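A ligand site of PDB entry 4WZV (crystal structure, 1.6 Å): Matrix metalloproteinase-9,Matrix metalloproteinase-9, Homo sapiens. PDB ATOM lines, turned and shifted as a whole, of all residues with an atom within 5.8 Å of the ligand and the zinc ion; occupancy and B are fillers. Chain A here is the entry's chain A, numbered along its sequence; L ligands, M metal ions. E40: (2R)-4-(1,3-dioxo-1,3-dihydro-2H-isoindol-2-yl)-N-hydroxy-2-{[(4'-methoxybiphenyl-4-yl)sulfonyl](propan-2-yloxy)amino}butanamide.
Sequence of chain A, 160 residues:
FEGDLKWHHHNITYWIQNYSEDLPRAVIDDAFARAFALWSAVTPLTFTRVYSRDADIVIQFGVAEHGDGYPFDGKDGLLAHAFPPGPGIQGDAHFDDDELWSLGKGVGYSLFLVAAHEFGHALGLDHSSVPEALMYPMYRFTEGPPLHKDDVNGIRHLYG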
ATOM      1  N   GLY A  77      -4.663  24.141  14.879  1.00  0.00           N
ATOM      2  CA  GLY A  77      -4.294  25.053  15.936  1.00  0.00           C
ATOM      3  C   GLY A  77      -3.718  24.294  17.114  1.00  0.00           C
ATOM      4  O   GLY A  77      -2.735  23.539  16.983  1.00  0.00           O
ATOM      5  N   LEU A  78      -4.325  24.491  18.274  1.00  0.00           N
ATOM      6  CA  LEU A  78      -3.825  23.889  19.494  1.00  0.00           C
ATOM      7  C   LEU A  78      -3.920  22.372  19.449  1.00  0.00           C
ATOM      8  O   LEU A  78      -4.896  21.828  18.926  1.00  0.00           O
ATOM      9  CB  LEU A  78      -4.583  24.423  20.705  1.00  0.00           C
ATOM     10  CG  LEU A  78      -4.324  25.850  21.185  1.00  0.00           C
ATOM     11  CD1 LEU A  78      -5.351  26.189  22.244  1.00  0.00           C
ATOM     12  CD2 LEU A  78      -2.918  26.038  21.740  1.00  0.00           C
ATOM     13  N   LEU A  79      -2.918  21.709  20.002  1.00  0.00           N
ATOM     14  CA  LEU A  79      -2.909  20.245  20.131  1.00  0.00           C
ATOM     15  C   LEU A  79      -3.189  19.781  21.561  1.00  0.00           C
ATOM     16  O   LEU A  79      -3.863  18.779  21.767  1.00  0.00           O
ATOM     17  CB  LEU A  79      -1.568  19.690  19.690  1.00  0.00           C
ATOM     18  CG  LEU A  79      -1.040  20.172  18.345  1.00  0.00           C
ATOM     19  CD1 LEU A  79       0.271  19.493  18.023  1.00  0.00           C
ATOM     20  CD2 LEU A  79      -2.069  19.837  17.281  1.00  0.00           C
ATOM     21  N   ALA A  80      -2.640  20.499  22.529  1.00  0.00           N
ATOM     22  CA  ALA A  80      -2.586  20.058  23.912  1.00  0.00           C
ATOM     23  C   ALA A  80      -2.053  21.223  24.713  1.00  0.00           C
ATOM     24  O   ALA A  80      -1.350  22.086  24.155  1.00  0.00           O
ATOM     25  CB  ALA A  80      -1.693  18.819  24.082  1.00  0.00           C
ATOM     26  N   HIS A  81      -2.380  21.278  26.001  1.00  0.00           N
ATOM     27  CA  HIS A  81      -1.680  22.230  26.860  1.00  0.00           C
ATOM     28  C   HIS A  81      -1.521  21.651  28.267  1.00  0.00           C
ATOM     29  O   HIS A  81      -2.266  20.761  28.649  1.00  0.00           O
ATOM     30  CB  HIS A  81      -2.386  23.603  26.902  1.00  0.00           C
ATOM     31  CG  HIS A  81      -3.806  23.588  27.376  1.00  0.00           C
ATOM     32  ND1 HIS A  81      -4.781  24.378  26.809  1.00  0.00           N
ATOM     33  CD2 HIS A  81      -4.409  22.902  28.376  1.00  0.00           C
ATOM     34  CE1 HIS A  81      -5.938  24.167  27.425  1.00  0.00           C
ATOM     35  NE2 HIS A  81      -5.739  23.273  28.375  1.00  0.00           N
ATOM     36  N   ALA A  82      -0.539  22.170  29.004  1.00  0.00           N
ATOM     37  CA  ALA A  82      -0.212  21.705  30.353  1.00  0.00           C
ATOM     38  C   ALA A  82       0.230  22.857  31.245  1.00  0.00           C
ATOM     39  O   ALA A  82       0.745  23.877  30.759  1.00  0.00           O
ATOM     40  CB  ALA A  82       0.889  20.633  30.309  1.00  0.00           C
ATOM     41  N   PHE A  83       0.045  22.688  32.547  1.00  0.00           N
ATOM     42  CA  PHE A  83       0.339  23.730  33.536  1.00  0.00           C
ATOM     43  C   PHE A  83       1.562  23.322  34.366  1.00  0.00           C
ATOM     44  O   PHE A  83       1.708  22.155  34.690  1.00  0.00           O
ATOM     45  CB  PHE A  83      -0.883  23.969  34.430  1.00  0.00           C
ATOM     46  CG  PHE A  83      -2.160  24.307  33.675  1.00  0.00           C
ATOM     47  CD1 PHE A  83      -2.925  23.310  33.066  1.00  0.00           C
ATOM     48  CD2 PHE A  83      -2.612  25.618  33.621  1.00  0.00           C
ATOM     49  CE1 PHE A  83      -4.095  23.632  32.382  1.00  0.00           C
ATOM     50  CE2 PHE A  83      -3.789  25.938  32.943  1.00  0.00           C
ATOM     51  CZ  PHE A  83      -4.536  24.951  32.326  1.00  0.00           C
ATOM     52  N   PRO A  84       2.462  24.280  34.676  1.00  0.00           N
ATOM     53  CA  PRO A  84       3.681  24.010  35.443  1.00  0.00           C
ATOM     54  C   PRO A  84       3.352  23.557  36.866  1.00  0.00           C
ATOM     55  O   PRO A  84       2.210  23.735  37.287  1.00  0.00           O
ATOM     56  CB  PRO A  84       4.420  25.360  35.438  1.00  0.00           C
ATOM     57  CG  PRO A  84       3.352  26.356  35.258  1.00  0.00           C
ATOM     58  CD  PRO A  84       2.324  25.708  34.363  1.00  0.00           C
ATOM     59  N   LEU A 113       4.550  11.449  21.608  1.00  0.00           N
ATOM     60  CA  LEU A 113       5.445  12.616  21.477  1.00  0.00           C
ATOM     61  C   LEU A 113       4.806  13.884  22.070  1.00  0.00           C
ATOM     62  O   LEU A 113       5.487  14.676  22.763  1.00  0.00           O
ATOM     63  CB  LEU A 113       5.814  12.824  20.010  1.00  0.00           C
ATOM     64  CG  LEU A 113       6.735  11.778  19.375  1.00  0.00           C
ATOM     65  CD1 LEU A 113       6.925  12.067  17.880  1.00  0.00           C
ATOM     66  CD2 LEU A 113       8.075  11.741  20.106  1.00  0.00           C
ATOM     67  N   VAL A 114       3.519  14.089  21.804  1.00  0.00           N
ATOM     68  CA  VAL A 114       2.833  15.263  22.320  1.00  0.00           C
ATOM     69  C   VAL A 114       2.759  15.176  23.843  1.00  0.00           C
ATOM     70  O   VAL A 114       3.011  16.165  24.529  1.00  0.00           O
ATOM     71  CB  VAL A 114       1.421  15.427  21.707  1.00  0.00           C
ATOM     72  CG1 VAL A 114       0.673  16.593  22.381  1.00  0.00           C
ATOM     73  CG2 VAL A 114       1.534  15.708  20.215  1.00  0.00           C
ATOM     74  N   HIS A 117       6.226  16.100  25.405  1.00  0.00           N
ATOM     75  CA  HIS A 117       6.330  17.562  25.432  1.00  0.00           C
ATOM     76  C   HIS A 117       5.463  18.155  26.549  1.00  0.00           C
ATOM     77  O   HIS A 117       5.937  19.006  27.299  1.00  0.00           O
ATOM     78  CB  HIS A 117       5.947  18.153  24.066  1.00  0.00           C
ATOM     79  CG  HIS A 117       5.928  19.650  24.024  1.00  0.00           C
ATOM     80  ND1 HIS A 117       6.960  20.411  23.508  1.00  0.00           N
ATOM     81  CD2 HIS A 117       4.956  20.525  24.362  1.00  0.00           C
ATOM     82  CE1 HIS A 117       6.636  21.695  23.545  1.00  0.00           C
ATOM     83  NE2 HIS A 117       5.427  21.791  24.084  1.00  0.00           N
ATOM     84  N   GLU A 118       4.194  17.729  26.654  1.00  0.00           N
ATOM     85  CA  GLU A 118       3.325  18.273  27.696  1.00  0.00           C
ATOM     86  C   GLU A 118       3.845  17.982  29.105  1.00  0.00           C
ATOM     87  O   GLU A 118       3.759  18.807  29.966  1.00  0.00           O
ATOM     88  CB  GLU A 118       1.888  17.732  27.569  1.00  0.00           C
ATOM     89  CG  GLU A 118       1.249  18.092  26.242  1.00  0.00           C
ATOM     90  CD  GLU A 118       1.288  19.582  25.974  1.00  0.00           C
ATOM     91  OE1 GLU A 118       1.028  20.335  26.928  1.00  0.00           O
ATOM     92  OE2 GLU A 118       1.655  19.971  24.837  1.00  0.00           O
ATOM     93  N   HIS A 121       6.346  20.386  30.306  1.00  0.00           N
ATOM     94  CA  HIS A 121       5.706  21.561  30.905  1.00  0.00           C
ATOM     95  C   HIS A 121       5.212  21.293  32.310  1.00  0.00           C
ATOM     96  O   HIS A 121       5.324  22.134  33.214  1.00  0.00           O
ATOM     97  CB  HIS A 121       4.496  22.007  30.085  1.00  0.00           C
ATOM     98  CG  HIS A 121       4.836  22.632  28.776  1.00  0.00           C
ATOM     99  ND1 HIS A 121       5.804  23.598  28.632  1.00  0.00           N
ATOM    100  CD2 HIS A 121       4.276  22.487  27.553  1.00  0.00           C
ATOM    101  CE1 HIS A 121       5.848  23.998  27.379  1.00  0.00           C
ATOM    102  NE2 HIS A 121       4.934  23.332  26.698  1.00  0.00           N
ATOM    103  N   LEU A 125       9.238  22.876  32.604  1.00  0.00           N
ATOM    104  CA  LEU A 125       9.955  23.415  31.454  1.00  0.00           C
ATOM    105  C   LEU A 125       9.092  24.334  30.602  1.00  0.00           C
ATOM    106  O   LEU A 125       7.934  24.024  30.312  1.00  0.00           O
ATOM    107  CB  LEU A 125      10.500  22.292  30.563  1.00  0.00           C
ATOM    108  CG  LEU A 125      11.575  21.397  31.201  1.00  0.00           C
ATOM    109  CD1 LEU A 125      12.131  20.453  30.123  1.00  0.00           C
ATOM    110  CD2 LEU A 125      12.681  22.224  31.832  1.00  0.00           C
ATOM    111  N   ASP A 126       9.654  25.483  30.216  1.00  0.00           N
ATOM    112  CA  ASP A 126       9.002  26.339  29.220  1.00  0.00           C
ATOM    113  C   ASP A 126       9.459  25.857  27.838  1.00  0.00           C
ATOM    114  O   ASP A 126      10.226  24.886  27.719  1.00  0.00           O
ATOM    115  CB  ASP A 126       9.393  27.811  29.449  1.00  0.00           C
ATOM    116  CG  ASP A 126       8.442  28.810  28.792  1.00  0.00           C
ATOM    117  OD1 ASP A 126       7.537  28.414  28.034  1.00  0.00           O
ATOM    118  OD2 ASP A 126       8.628  30.032  29.019  1.00  0.00           O
ATOM    119  N   HIS A 127       8.990  26.519  26.788  1.00  0.00           N
ATOM    120  CA  HIS A 127       9.473  26.185  25.456  1.00  0.00           C
ATOM    121  C   HIS A 127      10.936  26.529  25.261  1.00  0.00           C
ATOM    122  O   HIS A 127      11.419  27.553  25.742  1.00  0.00           O
ATOM    123  CB  HIS A 127       8.638  26.898  24.404  1.00  0.00           C
ATOM    124  CG  HIS A 127       7.253  26.338  24.254  1.00  0.00           C
ATOM    125  ND1 HIS A 127       6.166  27.116  23.954  1.00  0.00           N
ATOM    126  CD2 HIS A 127       6.797  25.064  24.351  1.00  0.00           C
ATOM    127  CE1 HIS A 127       5.087  26.349  23.901  1.00  0.00           C
ATOM    128  NE2 HIS A 127       5.456  25.098  24.120  1.00  0.00           N
ATOM    129  N   ALA A 133      14.512  20.419  19.726  1.00  0.00           N
ATOM    130  CA  ALA A 133      14.359  20.080  21.159  1.00  0.00           C
ATOM    131  C   ALA A 133      12.971  19.564  21.352  1.00  0.00           C
ATOM    132  O   ALA A 133      12.078  19.950  20.598  1.00  0.00           O
ATOM    133  CB  ALA A 133      14.628  21.278  22.052  1.00  0.00           C
ATOM    134  N   LEU A 134      12.777  18.643  22.298  1.00  0.00           N
ATOM    135  CA  LEU A 134      11.444  18.143  22.601  1.00  0.00           C
ATOM    136  C   LEU A 134      10.545  19.306  22.983  1.00  0.00           C
ATOM    137  O   LEU A 134       9.351  19.336  22.673  1.00  0.00           O
ATOM    138  CB  LEU A 134      11.476  17.105  23.709  1.00  0.00           C
ATOM    139  CG  LEU A 134      10.100  16.572  24.138  1.00  0.00           C
ATOM    140  CD1 LEU A 134       9.380  15.918  22.979  1.00  0.00           C
ATOM    141  CD2 LEU A 134      10.249  15.578  25.298  1.00  0.00           C
ATOM    142  N   MET A 135      11.135  20.268  23.691  1.00  0.00           N
ATOM    143  CA  MET A 135      10.389  21.401  24.208  1.00  0.00           C
ATOM    144  C   MET A 135      10.304  22.556  23.205  1.00  0.00           C
ATOM    145  O   MET A 135       9.710  23.573  23.468  1.00  0.00           O
ATOM    146  CB  MET A 135      10.989  21.891  25.544  1.00  0.00           C
ATOM    147  CG  MET A 135      10.815  20.934  26.731  1.00  0.00           C
ATOM    148  SD  MET A 135       9.194  20.128  26.850  1.00  0.00           S
ATOM    149  CE  MET A 135       8.028  21.489  26.906  1.00  0.00           C
ATOM    150  N   TYR A 136      10.924  22.398  22.037  1.00  0.00           N
ATOM    151  CA  TYR A 136      10.697  23.361  20.950  1.00  0.00           C
ATOM    152  C   TYR A 136       9.221  23.328  20.583  1.00  0.00           C
ATOM    153  O   TYR A 136       8.668  22.255  20.451  1.00  0.00           O
ATOM    154  CB  TYR A 136      11.542  22.996  19.742  1.00  0.00           C
ATOM    155  CG  TYR A 136      11.707  24.079  18.712  1.00  0.00           C
ATOM    156  CD1 TYR A 136      12.512  25.192  18.968  1.00  0.00           C
ATOM    157  CD2 TYR A 136      11.094  23.980  17.471  1.00  0.00           C
ATOM    158  CE1 TYR A 136      12.693  26.190  18.012  1.00  0.00           C
ATOM    159  CE2 TYR A 136      11.269  24.985  16.510  1.00  0.00           C
ATOM    160  CZ  TYR A 136      12.070  26.075  16.801  1.00  0.00           C
ATOM    161  OH  TYR A 136      12.252  27.087  15.880  1.00  0.00           O
ATOM    162  N   PRO A 137       8.583  24.503  20.409  1.00  0.00           N
ATOM    163  CA  PRO A 137       7.135  24.609  20.212  1.00  0.00           C
ATOM    164  C   PRO A 137       6.678  24.279  18.786  1.00  0.00           C
ATOM    165  O   PRO A 137       5.877  24.997  18.184  1.00  0.00           O
ATOM    166  CB  PRO A 137       6.861  26.085  20.534  1.00  0.00           C
ATOM    167  CG  PRO A 137       8.112  26.766  20.076  1.00  0.00           C
ATOM    168  CD  PRO A 137       9.224  25.825  20.502  1.00  0.00           C
ATOM    169  N   MET A 138       7.194  23.180  18.264  1.00  0.00           N
ATOM    170  CA  MET A 138       6.825  22.699  16.946  1.00  0.00           C
ATOM    171  C   MET A 138       6.686  21.200  16.992  1.00  0.00           C
ATOM    172  O   MET A 138       7.644  20.482  17.300  1.00  0.00           O
ATOM    173  CB  MET A 138       7.858  23.096  15.902  1.00  0.00           C
ATOM    174  CG  MET A 138       7.688  22.344  14.574  1.00  0.00           C
ATOM    175  SD  MET A 138       7.711  23.456  13.165  1.00  0.00           S
ATOM    176  CE  MET A 138       6.280  24.457  13.522  1.00  0.00           C
ATOM    177  N   TYR A 139       5.476  20.713  16.708  1.00  0.00           N
ATOM    178  CA  TYR A 139       5.276  19.285  16.581  1.00  0.00           C
ATOM    179  C   TYR A 139       5.969  18.767  15.349  1.00  0.00           C
ATOM    180  O   TYR A 139       5.793  19.308  14.263  1.00  0.00           O
ATOM    181  CB  TYR A 139       3.781  18.940  16.483  1.00  0.00           C
ATOM    182  CG  TYR A 139       3.620  17.478  16.271  1.00  0.00           C
ATOM    183  CD1 TYR A 139       3.649  16.598  17.338  1.00  0.00           C
ATOM    184  CD2 TYR A 139       3.514  16.948  14.977  1.00  0.00           C
ATOM    185  CE1 TYR A 139       3.534  15.224  17.138  1.00  0.00           C
ATOM    186  CE2 TYR A 139       3.421  15.592  14.775  1.00  0.00           C
ATOM    187  CZ  TYR A 139       3.420  14.735  15.845  1.00  0.00           C
ATOM    188  OH  TYR A 139       3.305  13.398  15.593  1.00  0.00           O
ATOM    189  N   ARG A 140       6.749  17.707  15.495  1.00  0.00           N
ATOM    190  CA  ARG A 140       7.227  17.002  14.326  1.00  0.00           C
ATOM    191  C   ARG A 140       7.301  15.532  14.664  1.00  0.00           C
ATOM    192  O   ARG A 140       7.740  15.188  15.757  1.00  0.00           O
ATOM    193  CB  ARG A 140       8.577  17.537  13.853  1.00  0.00           C
ATOM    194  CG  ARG A 140       8.959  17.033  12.473  1.00  0.00           C
ATOM    195  CD  ARG A 140       9.921  17.972  11.783  1.00  0.00           C
ATOM    196  NE  ARG A 140       9.399  19.333  11.754  1.00  0.00           N
ATOM    197  CZ  ARG A 140      10.146  20.414  11.557  1.00  0.00           C
ATOM    198  NH1 ARG A 140      11.446  20.292  11.387  1.00  0.00           N
ATOM    199  NH2 ARG A 140       9.584  21.608  11.550  1.00  0.00           N
HETATM  200  O13 E40 L   1       0.211  24.042  19.320  1.00  0.00           O
HETATM  201  S13 E40 L   1       0.374  23.695  20.726  1.00  0.00           S
HETATM  202  O14 E40 L   1      -0.849  23.083  21.233  1.00  0.00           O
HETATM  203  C28 E40 L   1       1.748  22.532  20.724  1.00  0.00           C
HETATM  204  C14 E40 L   1       2.805  22.729  19.840  1.00  0.00           C
HETATM  205  C17 E40 L   1       3.847  21.819  19.785  1.00  0.00           C
HETATM  206  C16 E40 L   1       3.842  20.713  20.624  1.00  0.00           C
HETATM  207  C21 E40 L   1       4.950  19.688  20.492  1.00  0.00           C
HETATM  208  C26 E40 L   1       6.390  20.142  20.282  1.00  0.00           C
HETATM  209  C25 E40 L   1       7.338  19.252  20.127  1.00  0.00           C
HETATM  210  C24 E40 L   1       6.978  17.768  20.098  1.00  0.00           C
HETATM  211  O24 E40 L   1       7.981  16.823  19.913  1.00  0.00           O
HETATM  212  C61 E40 L   1       9.193  17.239  19.379  1.00  0.00           C
HETATM  213  C23 E40 L   1       5.725  17.373  20.242  1.00  0.00           C
HETATM  214  C30 E40 L   1       4.627  18.414  20.419  1.00  0.00           C
HETATM  215  C15 E40 L   1       2.790  20.511  21.495  1.00  0.00           C
HETATM  216  C29 E40 L   1       1.752  21.415  21.538  1.00  0.00           C
HETATM  217  N12 E40 L   1       0.688  25.110  21.631  1.00  0.00           N
HETATM  218  O15 E40 L   1       1.924  25.656  21.320  1.00  0.00           O
HETATM  219  C67 E40 L   1       2.003  26.621  20.288  1.00  0.00           C
HETATM  220  C69 E40 L   1       3.455  27.026  20.141  1.00  0.00           C
HETATM  221  C68 E40 L   1       1.188  27.866  20.632  1.00  0.00           C
HETATM  222  C31 E40 L   1       0.518  24.920  23.065  1.00  0.00           C
HETATM  223  C11 E40 L   1       1.687  24.166  23.722  1.00  0.00           C
HETATM  224  O2  E40 L   1       2.773  24.646  23.776  1.00  0.00           O
HETATM  225  N2  E40 L   1       1.440  22.935  24.441  1.00  0.00           N
HETATM  226  O7  E40 L   1       2.548  22.279  24.977  1.00  0.00           O
HETATM  227  C32 E40 L   1       0.416  26.316  23.636  1.00  0.00           C
HETATM  228  C33 E40 L   1      -0.040  26.214  25.078  1.00  0.00           C
HETATM  229  N48 E40 L   1       1.092  26.219  25.980  1.00  0.00           N
HETATM  230  C52 E40 L   1       1.258  25.365  27.132  1.00  0.00           C
HETATM  231  O54 E40 L   1       0.553  24.456  27.446  1.00  0.00           O
HETATM  232  C49 E40 L   1       2.181  27.176  26.015  1.00  0.00           C
HETATM  233  O53 E40 L   1       2.397  28.062  25.253  1.00  0.00           O
HETATM  234  C50 E40 L   1       3.040  26.862  27.220  1.00  0.00           C
HETATM  235  C51 E40 L   1       2.507  25.829  27.865  1.00  0.00           C
HETATM  236  C55 E40 L   1       4.302  27.542  27.731  1.00  0.00           C
HETATM  237  C56 E40 L   1       4.876  27.088  28.827  1.00  0.00           C
HETATM  238  C57 E40 L   1       4.255  25.906  29.550  1.00  0.00           C
HETATM  239  C58 E40 L   1       3.168  25.317  29.120  1.00  0.00           C
HETATM  240 ZN    ZN M   1       4.296  23.447  24.599  1.00  0.00          ZN
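The side-chain carboxylate of Glu 118 is in hydrogen-bond range of a nitrogen (N2) of the ligand (3.0 Å). The backbone NH (N) of Leu 79 lies within hydrogen-bond range of an oxygen (O14) of the ligand, at 2.8 Å. N of Ala 80 lies within hydrogen-bond range of O14 of the ligand (3.4 Å). O of Ala 80 sits at hydrogen-bond distance from N2 of the ligand, at 2.9 Å. O54 of the ligand sits at hydrogen-bond distance from N of Ala 82 (3.0 Å).
The backbone carbonyl oxygen (O) of Leu 134 is in hydrogen-bond range of a ring nitrogen (ND1) of His 117 (2.8 Å). The backbone carbonyl oxygen of Leu 125 is in hydrogen-bond range of a ring nitrogen (ND1) of His 121, at 2.7 Å. OE1 of Glu 118 lies within hydrogen-bond range of N of Ala 82 (3.2 Å). The guanidinium group of Arg 140 is in hydrogen-bond range of the side-chain sulfur of Met 138 (3.1 Å).
Residues that only touch the ligand: Asp 126, Met 138, His 81, Tyr 136, Leu 134, Leu 78, Pro 137, Tyr 139, Leu 113 and Gly 77. Hydrophobic or aromatic side chains within 4 Å of the ligand: Leu 78, Leu 79, His 81, His 117, His 121, His 127, Leu 134, Pro 137 and Tyr 139. Along chain A the residues within 4 Å of the ligand span positions 77 to 139.
Three residues have an atom within 4 Å of the zinc ion: His 117, His 121 and His 127.
The zinc ion is bound by NE2 of His 117 (2.1 Å), NE2 of His 127 (2.1 Å), O2 of the ligand (2.1 Å), O7 of the ligand (2.1 Å) and NE2 of His 121 (2.2 Å). The zinc ion has five donor atoms within binding distance.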
